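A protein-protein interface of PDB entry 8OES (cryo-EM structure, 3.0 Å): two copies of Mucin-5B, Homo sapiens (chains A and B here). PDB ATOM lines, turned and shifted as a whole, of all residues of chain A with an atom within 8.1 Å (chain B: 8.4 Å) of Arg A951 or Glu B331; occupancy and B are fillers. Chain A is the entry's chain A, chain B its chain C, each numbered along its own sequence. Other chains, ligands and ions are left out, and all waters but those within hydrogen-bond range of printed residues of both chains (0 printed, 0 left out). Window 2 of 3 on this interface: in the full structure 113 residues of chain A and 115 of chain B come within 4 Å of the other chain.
No position is printed for both chains. Of the 3 pairs that touch across the chains among the printed residues, none has its exchanged pair printed and touching as well.
Of the printed residues of chain B, Arg A911 touches Leu B329. Of the printed residues of chain B, Phe A933 touches Leu B329 (3.6 Å). Val A949 touches none of the printed residues of chain B. Arg A951 touches one residue of chain B. No residue of chain B comes within 4 Å of Gly A952. Printed residues of chain A within 4 Å of Leu B329: Arg A911 and Phe A933. Glu B331 touches just one residue of chain A: Arg A951 (3.2 Å). The nearest residue of chain B that does not touch Arg A951 is Ala B46 (4.5 Å). The nearest residue of chain A that does not touch Glu B331 is Val A949 (4.9 Å). The nearest printed residue of chain B that does not touch Arg A911 is Cys B330 (5.0 Å).
Of the 15 printed residues of chain A, 3 touch a printed residue of chain B. Hydrophobic or aromatic side chains of chain A within 4 Å of the printed part of chain B: Phe A933. Printed residues of chain B that touch a printed residue of chain A: Leu B329 and Glu B331. Hydrophobic or aromatic side chains of chain B that line the printed part of chain A: Leu B329. Among the printed residues, Asp or Glu carboxylates within 4 Å of a Lys or Arg side-chain nitrogen of the other chain: Arg A951 with Glu B331 (3.2 Å).
Among the printed residues, merely in contact across the chains: Arg A911 with Leu B329 (3.6 Å) and Phe A933 with Leu B329 (3.6 Å).
SG of Cys B317 forms a disulfide with SG of Cys B330 (2.0 Å). O of Arg A911 is in hydrogen-bond range of N of Phe A933, 2.8 Å away.
The guanidinium group of Arg A951 lies within salt-bridge range of the side-chain carboxylate of Glu B331.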
ATOM      1  N   ARG A 911     -14.617  22.330 -22.350  1.00  0.00           N
ATOM      2  CA  ARG A 911     -15.929  21.705 -22.315  1.00  0.00           C
ATOM      3  C   ARG A 911     -16.384  21.538 -20.875  1.00  0.00           C
ATOM      4  O   ARG A 911     -15.619  21.055 -20.039  1.00  0.00           O
ATOM      5  CB  ARG A 911     -15.890  20.352 -23.008  1.00  0.00           C
ATOM      6  CG  ARG A 911     -17.196  19.949 -23.604  1.00  0.00           C
ATOM      7  CD  ARG A 911     -17.904  18.941 -22.743  1.00  0.00           C
ATOM      8  NE  ARG A 911     -17.288  17.629 -22.840  1.00  0.00           N
ATOM      9  CZ  ARG A 911     -17.337  16.859 -23.916  1.00  0.00           C
ATOM     10  NH1 ARG A 911     -17.984  17.234 -25.006  1.00  0.00           N
ATOM     11  NH2 ARG A 911     -16.724  15.680 -23.897  1.00  0.00           N
ATOM     12  N   LYS A 931     -17.924  18.566 -14.971  1.00  0.00           N
ATOM     13  CA  LYS A 931     -16.801  17.934 -15.662  1.00  0.00           C
ATOM     14  C   LYS A 931     -16.079  18.984 -16.499  1.00  0.00           C
ATOM     15  O   LYS A 931     -16.339  19.131 -17.693  1.00  0.00           O
ATOM     16  CB  LYS A 931     -17.276  16.775 -16.499  1.00  0.00           C
ATOM     17  CG  LYS A 931     -17.713  15.591 -15.671  1.00  0.00           C
ATOM     18  CD  LYS A 931     -18.171  14.458 -16.554  1.00  0.00           C
ATOM     19  CE  LYS A 931     -18.438  13.211 -15.746  1.00  0.00           C
ATOM     20  NZ  LYS A 931     -19.134  12.181 -16.562  1.00  0.00           N
ATOM     21  N   PHE A 933     -13.506  19.802 -18.600  1.00  0.00           N
ATOM     22  CA  PHE A 933     -12.451  19.370 -19.503  1.00  0.00           C
ATOM     23  C   PHE A 933     -11.708  20.601 -19.994  1.00  0.00           C
ATOM     24  O   PHE A 933     -12.321  21.633 -20.271  1.00  0.00           O
ATOM     25  CB  PHE A 933     -13.002  18.598 -20.700  1.00  0.00           C
ATOM     26  CG  PHE A 933     -13.859  17.417 -20.346  1.00  0.00           C
ATOM     27  CD1 PHE A 933     -13.954  16.954 -19.058  1.00  0.00           C
ATOM     28  CD2 PHE A 933     -14.557  16.754 -21.334  1.00  0.00           C
ATOM     29  CE1 PHE A 933     -14.748  15.871 -18.761  1.00  0.00           C
ATOM     30  CE2 PHE A 933     -15.342  15.670 -21.039  1.00  0.00           C
ATOM     31  CZ  PHE A 933     -15.435  15.227 -19.754  1.00  0.00           C
ATOM     32  N   SER A 936      -6.704  18.260 -23.105  1.00  0.00           N
ATOM     33  CA  SER A 936      -6.527  16.856 -22.757  1.00  0.00           C
ATOM     34  C   SER A 936      -6.656  16.584 -21.267  1.00  0.00           C
ATOM     35  O   SER A 936      -6.619  15.419 -20.861  1.00  0.00           O
ATOM     36  CB  SER A 936      -5.169  16.355 -23.249  1.00  0.00           C
ATOM     37  OG  SER A 936      -5.112  16.345 -24.662  1.00  0.00           O
ATOM     38  N   TYR A 937      -6.815  17.613 -20.447  1.00  0.00           N
ATOM     39  CA  TYR A 937      -7.001  17.413 -19.021  1.00  0.00           C
ATOM     40  C   TYR A 937      -8.462  17.112 -18.726  1.00  0.00           C
ATOM     41  O   TYR A 937      -9.271  16.884 -19.626  1.00  0.00           O
ATOM     42  CB  TYR A 937      -6.536  18.623 -18.217  1.00  0.00           C
ATOM     43  CG  TYR A 937      -5.043  18.771 -18.079  1.00  0.00           C
ATOM     44  CD1 TYR A 937      -4.179  18.366 -19.080  1.00  0.00           C
ATOM     45  CD2 TYR A 937      -4.500  19.262 -16.907  1.00  0.00           C
ATOM     46  CE1 TYR A 937      -2.819  18.492 -18.931  1.00  0.00           C
ATOM     47  CE2 TYR A 937      -3.151  19.381 -16.745  1.00  0.00           C
ATOM     48  CZ  TYR A 937      -2.314  19.003 -17.756  1.00  0.00           C
ATOM     49  OH  TYR A 937      -0.961  19.134 -17.577  1.00  0.00           O
ATOM     50  N   GLU A 938      -8.805  17.104 -17.443  1.00  0.00           N
ATOM     51  CA  GLU A 938     -10.153  16.810 -16.997  1.00  0.00           C
ATOM     52  C   GLU A 938     -10.207  17.096 -15.508  1.00  0.00           C
ATOM     53  O   GLU A 938      -9.231  16.841 -14.804  1.00  0.00           O
ATOM     54  CB  GLU A 938     -10.501  15.348 -17.285  1.00  0.00           C
ATOM     55  CG  GLU A 938     -11.936  14.993 -17.106  1.00  0.00           C
ATOM     56  CD  GLU A 938     -12.318  14.928 -15.674  1.00  0.00           C
ATOM     57  OE1 GLU A 938     -13.366  15.491 -15.319  1.00  0.00           O
ATOM     58  OE2 GLU A 938     -11.549  14.348 -14.894  1.00  0.00           O
ATOM     59  N   ILE A 940     -13.219  16.565 -12.382  1.00  0.00           N
ATOM     60  CA  ILE A 940     -14.561  16.253 -11.910  1.00  0.00           C
ATOM     61  C   ILE A 940     -14.780  17.000 -10.605  1.00  0.00           C
ATOM     62  O   ILE A 940     -13.975  16.889  -9.674  1.00  0.00           O
ATOM     63  CB  ILE A 940     -14.764  14.748 -11.713  1.00  0.00           C
ATOM     64  CG1 ILE A 940     -14.180  13.969 -12.875  1.00  0.00           C
ATOM     65  CG2 ILE A 940     -16.228  14.449 -11.713  1.00  0.00           C
ATOM     66  CD1 ILE A 940     -14.247  12.480 -12.691  1.00  0.00           C
ATOM     67  N   ALA A 948      -8.852  14.941 -10.464  1.00  0.00           N
ATOM     68  CA  ALA A 948      -8.097  15.129 -11.693  1.00  0.00           C
ATOM     69  C   ALA A 948      -7.925  13.770 -12.340  1.00  0.00           C
ATOM     70  O   ALA A 948      -7.387  12.848 -11.722  1.00  0.00           O
ATOM     71  CB  ALA A 948      -6.743  15.782 -11.424  1.00  0.00           C
ATOM     72  N   VAL A 949      -8.394  13.644 -13.571  1.00  0.00           N
ATOM     73  CA  VAL A 949      -8.320  12.387 -14.297  1.00  0.00           C
ATOM     74  C   VAL A 949      -7.541  12.664 -15.576  1.00  0.00           C
ATOM     75  O   VAL A 949      -7.912  12.200 -16.657  1.00  0.00           O
ATOM     76  CB  VAL A 949      -9.720  11.806 -14.568  1.00  0.00           C
ATOM     77  CG1 VAL A 949      -9.635  10.377 -15.104  1.00  0.00           C
ATOM     78  CG2 VAL A 949     -10.551  11.843 -13.302  1.00  0.00           C
ATOM     79  N   ALA A 950      -6.519  13.513 -15.477  1.00  0.00           N
ATOM     80  CA  ALA A 950      -5.690  13.841 -16.631  1.00  0.00           C
ATOM     81  C   ALA A 950      -5.247  12.582 -17.368  1.00  0.00           C
ATOM     82  O   ALA A 950      -4.526  11.746 -16.816  1.00  0.00           O
ATOM     83  CB  ALA A 950      -4.472  14.648 -16.179  1.00  0.00           C
ATOM     84  N   ARG A 951      -5.691  12.450 -18.617  1.00  0.00           N
ATOM     85  CA  ARG A 951      -5.402  11.278 -19.432  1.00  0.00           C
ATOM     86  C   ARG A 951      -4.473  11.556 -20.598  1.00  0.00           C
ATOM     87  O   ARG A 951      -3.706  10.669 -20.980  1.00  0.00           O
ATOM     88  CB  ARG A 951      -6.701  10.674 -19.992  1.00  0.00           C
ATOM     89  CG  ARG A 951      -7.739  10.334 -18.944  1.00  0.00           C
ATOM     90  CD  ARG A 951      -7.832   8.846 -18.667  1.00  0.00           C
ATOM     91  NE  ARG A 951      -8.049   8.073 -19.883  1.00  0.00           N
ATOM     92  CZ  ARG A 951      -8.384   6.791 -19.904  1.00  0.00           C
ATOM     93  NH1 ARG A 951      -8.558   6.103 -18.787  1.00  0.00           N
ATOM     94  NH2 ARG A 951      -8.553   6.185 -21.076  1.00  0.00           N
ATOM     95  N   GLY A 952      -4.522  12.751 -21.178  1.00  0.00           N
ATOM     96  CA  GLY A 952      -3.768  13.050 -22.371  1.00  0.00           C
ATOM     97  C   GLY A 952      -2.325  13.416 -22.093  1.00  0.00           C
ATOM     98  O   GLY A 952      -1.703  12.924 -21.145  1.00  0.00           O
ATOM     99  N   PRO A 953      -1.758  14.273 -22.950  1.00  0.00           N
ATOM    100  CA  PRO A 953      -0.388  14.763 -22.725  1.00  0.00           C
ATOM    101  C   PRO A 953      -0.188  15.365 -21.342  1.00  0.00           C
ATOM    102  O   PRO A 953      -0.950  16.237 -20.917  1.00  0.00           O
ATOM    103  CB  PRO A 953      -0.209  15.820 -23.820  1.00  0.00           C
ATOM    104  CG  PRO A 953      -1.188  15.452 -24.889  1.00  0.00           C
ATOM    105  CD  PRO A 953      -2.258  14.580 -24.299  1.00  0.00           C
ATOM    106  N   GLY A 954       0.839  14.900 -20.636  1.00  0.00           N
ATOM    107  CA  GLY A 954       1.079  15.315 -19.269  1.00  0.00           C
ATOM    108  C   GLY A 954       2.009  16.498 -19.085  1.00  0.00           C
ATOM    109  O   GLY A 954       3.134  16.337 -18.602  1.00  0.00           O
ATOM    110  N   ASP A1199      -0.246  15.691 -10.295  1.00  0.00           N
ATOM    111  CA  ASP A1199      -1.666  15.434 -10.090  1.00  0.00           C
ATOM    112  C   ASP A1199      -2.288  16.395  -9.089  1.00  0.00           C
ATOM    113  O   ASP A1199      -3.511  16.562  -9.088  1.00  0.00           O
ATOM    114  CB  ASP A1199      -1.881  13.990  -9.633  1.00  0.00           C
ATOM    115  CG  ASP A1199      -1.736  12.989 -10.766  1.00  0.00           C
ATOM    116  OD1 ASP A1199      -1.874  13.390 -11.942  1.00  0.00           O
ATOM    117  OD2 ASP A1199      -1.478  11.801 -10.480  1.00  0.00           O
ATOM    118  N   ALA B  46      -7.808   3.418 -14.657  1.00  0.00           N
ATOM    119  CA  ALA B  46      -9.201   3.130 -14.969  1.00  0.00           C
ATOM    120  C   ALA B  46      -9.853   2.307 -13.864  1.00  0.00           C
ATOM    121  O   ALA B  46      -9.460   2.389 -12.702  1.00  0.00           O
ATOM    122  CB  ALA B  46      -9.311   2.403 -16.299  1.00  0.00           C
ATOM    123  N   HIS B  47     -10.844   1.499 -14.242  1.00  0.00           N
ATOM    124  CA  HIS B  47     -11.579   0.663 -13.294  1.00  0.00           C
ATOM    125  C   HIS B  47     -10.713  -0.530 -12.898  1.00  0.00           C
ATOM    126  O   HIS B  47     -10.993  -1.689 -13.210  1.00  0.00           O
ATOM    127  CB  HIS B  47     -12.895   0.213 -13.905  1.00  0.00           C
ATOM    128  CG  HIS B  47     -13.754   1.344 -14.359  1.00  0.00           C
ATOM    129  ND1 HIS B  47     -14.774   1.184 -15.270  1.00  0.00           N
ATOM    130  CD2 HIS B  47     -13.746   2.656 -14.025  1.00  0.00           C
ATOM    131  CE1 HIS B  47     -15.358   2.351 -15.480  1.00  0.00           C
ATOM    132  NE2 HIS B  47     -14.754   3.260 -14.736  1.00  0.00           N
ATOM    133  N   HIS B 286     -11.936  -3.685 -18.459  1.00  0.00           N
ATOM    134  CA  HIS B 286     -12.109  -2.855 -17.271  1.00  0.00           C
ATOM    135  C   HIS B 286     -10.780  -2.473 -16.630  1.00  0.00           C
ATOM    136  O   HIS B 286     -10.671  -1.392 -16.042  1.00  0.00           O
ATOM    137  CB  HIS B 286     -12.998  -3.570 -16.259  1.00  0.00           C
ATOM    138  CG  HIS B 286     -14.427  -3.150 -16.328  1.00  0.00           C
ATOM    139  ND1 HIS B 286     -15.340  -3.755 -17.161  1.00  0.00           N
ATOM    140  CD2 HIS B 286     -15.094  -2.161 -15.692  1.00  0.00           C
ATOM    141  CE1 HIS B 286     -16.515  -3.171 -17.020  1.00  0.00           C
ATOM    142  NE2 HIS B 286     -16.392  -2.198 -16.136  1.00  0.00           N
ATOM    143  N   ALA B 287      -9.775  -3.339 -16.711  1.00  0.00           N
ATOM    144  CA  ALA B 287      -8.461  -2.960 -16.210  1.00  0.00           C
ATOM    145  C   ALA B 287      -7.871  -1.829 -17.038  1.00  0.00           C
ATOM    146  O   ALA B 287      -7.156  -0.973 -16.511  1.00  0.00           O
ATOM    147  CB  ALA B 287      -7.526  -4.166 -16.204  1.00  0.00           C
ATOM    148  N   GLY B 288      -8.154  -1.816 -18.337  1.00  0.00           N
ATOM    149  CA  GLY B 288      -7.665  -0.765 -19.205  1.00  0.00           C
ATOM    150  C   GLY B 288      -7.175  -1.270 -20.547  1.00  0.00           C
ATOM    151  O   GLY B 288      -7.115  -0.509 -21.516  1.00  0.00           O
ATOM    152  N   PRO B 316     -17.585   2.981 -26.263  1.00  0.00           N
ATOM    153  CA  PRO B 316     -18.904   2.911 -25.613  1.00  0.00           C
ATOM    154  C   PRO B 316     -19.890   3.935 -26.118  1.00  0.00           C
ATOM    155  O   PRO B 316     -21.092   3.656 -26.176  1.00  0.00           O
ATOM    156  CB  PRO B 316     -18.568   3.159 -24.140  1.00  0.00           C
ATOM    157  CG  PRO B 316     -17.353   4.002 -24.193  1.00  0.00           C
ATOM    158  CD  PRO B 316     -16.555   3.528 -25.367  1.00  0.00           C
ATOM    159  N   CYS B 317     -19.415   5.125 -26.469  1.00  0.00           N
ATOM    160  CA  CYS B 317     -20.278   6.224 -26.888  1.00  0.00           C
ATOM    161  C   CYS B 317     -20.394   6.190 -28.405  1.00  0.00           C
ATOM    162  O   CYS B 317     -19.577   6.761 -29.129  1.00  0.00           O
ATOM    163  CB  CYS B 317     -19.725   7.545 -26.376  1.00  0.00           C
ATOM    164  SG  CYS B 317     -17.938   7.690 -26.480  1.00  0.00           S
ATOM    165  N   ARG B 326     -20.351  12.724 -30.201  1.00  0.00           N
ATOM    166  CA  ARG B 326     -20.347  12.316 -28.801  1.00  0.00           C
ATOM    167  C   ARG B 326     -19.056  11.594 -28.456  1.00  0.00           C
ATOM    168  O   ARG B 326     -18.515  11.760 -27.358  1.00  0.00           O
ATOM    169  CB  ARG B 326     -21.562  11.431 -28.516  1.00  0.00           C
ATOM    170  CG  ARG B 326     -21.428  10.465 -27.348  1.00  0.00           C
ATOM    171  CD  ARG B 326     -21.310  11.178 -26.012  1.00  0.00           C
ATOM    172  NE  ARG B 326     -21.339  10.249 -24.889  1.00  0.00           N
ATOM    173  CZ  ARG B 326     -20.660  10.413 -23.760  1.00  0.00           C
ATOM    174  NH1 ARG B 326     -19.859  11.450 -23.578  1.00  0.00           N
ATOM    175  NH2 ARG B 326     -20.790   9.514 -22.789  1.00  0.00           N
ATOM    176  N   ALA B 327     -18.521  10.829 -29.400  1.00  0.00           N
ATOM    177  CA  ALA B 327     -17.332  10.024 -29.170  1.00  0.00           C
ATOM    178  C   ALA B 327     -16.043  10.835 -29.227  1.00  0.00           C
ATOM    179  O   ALA B 327     -14.968  10.250 -29.397  1.00  0.00           O
ATOM    180  CB  ALA B 327     -17.274   8.877 -30.180  1.00  0.00           C
ATOM    181  N   GLN B 328     -16.117  12.159 -29.090  1.00  0.00           N
ATOM    182  CA  GLN B 328     -14.919  12.981 -29.214  1.00  0.00           C
ATOM    183  C   GLN B 328     -14.012  12.828 -27.999  1.00  0.00           C
ATOM    184  O   GLN B 328     -12.886  12.330 -28.108  1.00  0.00           O
ATOM    185  CB  GLN B 328     -15.308  14.445 -29.410  1.00  0.00           C
ATOM    186  CG  GLN B 328     -14.114  15.373 -29.556  1.00  0.00           C
ATOM    187  CD  GLN B 328     -14.218  16.279 -30.761  1.00  0.00           C
ATOM    188  OE1 GLN B 328     -14.806  15.922 -31.777  1.00  0.00           O
ATOM    189  NE2 GLN B 328     -13.630  17.460 -30.656  1.00  0.00           N
ATOM    190  N   LEU B 329     -14.487  13.239 -26.829  1.00  0.00           N
ATOM    191  CA  LEU B 329     -13.670  13.268 -25.619  1.00  0.00           C
ATOM    192  C   LEU B 329     -14.311  12.413 -24.535  1.00  0.00           C
ATOM    193  O   LEU B 329     -14.435  12.811 -23.375  1.00  0.00           O
ATOM    194  CB  LEU B 329     -13.449  14.705 -25.151  1.00  0.00           C
ATOM    195  CG  LEU B 329     -12.321  14.957 -24.149  1.00  0.00           C
ATOM    196  CD1 LEU B 329     -11.041  14.324 -24.640  1.00  0.00           C
ATOM    197  CD2 LEU B 329     -12.114  16.442 -23.931  1.00  0.00           C
ATOM    198  N   CYS B 330     -14.738  11.213 -24.914  1.00  0.00           N
ATOM    199  CA  CYS B 330     -15.354  10.293 -23.973  1.00  0.00           C
ATOM    200  C   CYS B 330     -14.330   9.799 -22.962  1.00  0.00           C
ATOM    201  O   CYS B 330     -13.123   9.769 -23.212  1.00  0.00           O
ATOM    202  CB  CYS B 330     -15.968   9.102 -24.700  1.00  0.00           C
ATOM    203  SG  CYS B 330     -17.542   9.416 -25.493  1.00  0.00           S
ATOM    204  N   GLU B 331     -14.832   9.403 -21.798  1.00  0.00           N
ATOM    205  CA  GLU B 331     -14.040   8.618 -20.869  1.00  0.00           C
ATOM    206  C   GLU B 331     -14.875   7.420 -20.460  1.00  0.00           C
ATOM    207  O   GLU B 331     -15.791   7.551 -19.651  1.00  0.00           O
ATOM    208  CB  GLU B 331     -13.618   9.438 -19.644  1.00  0.00           C
ATOM    209  CG  GLU B 331     -12.372   8.910 -18.925  1.00  0.00           C
ATOM    210  CD  GLU B 331     -12.565   7.559 -18.250  1.00  0.00           C
ATOM    211  OE1 GLU B 331     -13.705   7.234 -17.866  1.00  0.00           O
ATOM    212  OE2 GLU B 331     -11.570   6.818 -18.106  1.00  0.00           O
ATOM    213  N   ASP B 332     -14.572   6.280 -21.076  1.00  0.00           N
ATOM    214  CA  ASP B 332     -15.054   4.941 -20.752  1.00  0.00           C
ATOM    215  C   ASP B 332     -14.266   3.939 -21.580  1.00  0.00           C
ATOM    216  O   ASP B 332     -13.986   4.177 -22.758  1.00  0.00           O
ATOM    217  CB  ASP B 332     -16.556   4.778 -20.998  1.00  0.00           C
ATOM    218  CG  ASP B 332     -17.405   5.198 -19.813  1.00  0.00           C
ATOM    219  OD1 ASP B 332     -16.844   5.409 -18.719  1.00  0.00           O
ATOM    220  OD2 ASP B 332     -18.639   5.305 -19.975  1.00  0.00           O
ATOM    221  N   HIS B 333     -13.922   2.811 -20.974  1.00  0.00           N
ATOM    222  CA  HIS B 333     -13.041   1.830 -21.588  1.00  0.00           C
ATOM    223  C   HIS B 333     -13.769   1.113 -22.722  1.00  0.00           C
ATOM    224  O   HIS B 333     -14.909   1.435 -23.072  1.00  0.00           O
ATOM    225  CB  HIS B 333     -12.551   0.860 -20.523  1.00  0.00           C
ATOM    226  CG  HIS B 333     -13.631   0.404 -19.594  1.00  0.00           C
ATOM    227  ND1 HIS B 333     -14.484  -0.632 -19.897  1.00  0.00           N
ATOM    228  CD2 HIS B 333     -14.008   0.858 -18.376  1.00  0.00           C
ATOM    229  CE1 HIS B 333     -15.337  -0.804 -18.904  1.00  0.00           C
ATOM    230  NE2 HIS B 333     -15.068   0.088 -17.967  1.00  0.00           N
ATOM    231  N   CYS B 334     -13.100   0.128 -23.319  1.00  0.00           N
ATOM    232  CA  CYS B 334     -13.747  -0.738 -24.291  1.00  0.00           C
ATOM    233  C   CYS B 334     -15.051  -1.291 -23.740  1.00  0.00           C
ATOM    234  O   CYS B 334     -15.176  -1.573 -22.547  1.00  0.00           O
ATOM    235  CB  CYS B 334     -12.837  -1.909 -24.664  1.00  0.00           C
ATOM    236  SG  CYS B 334     -11.223  -1.517 -25.322  1.00  0.00           S
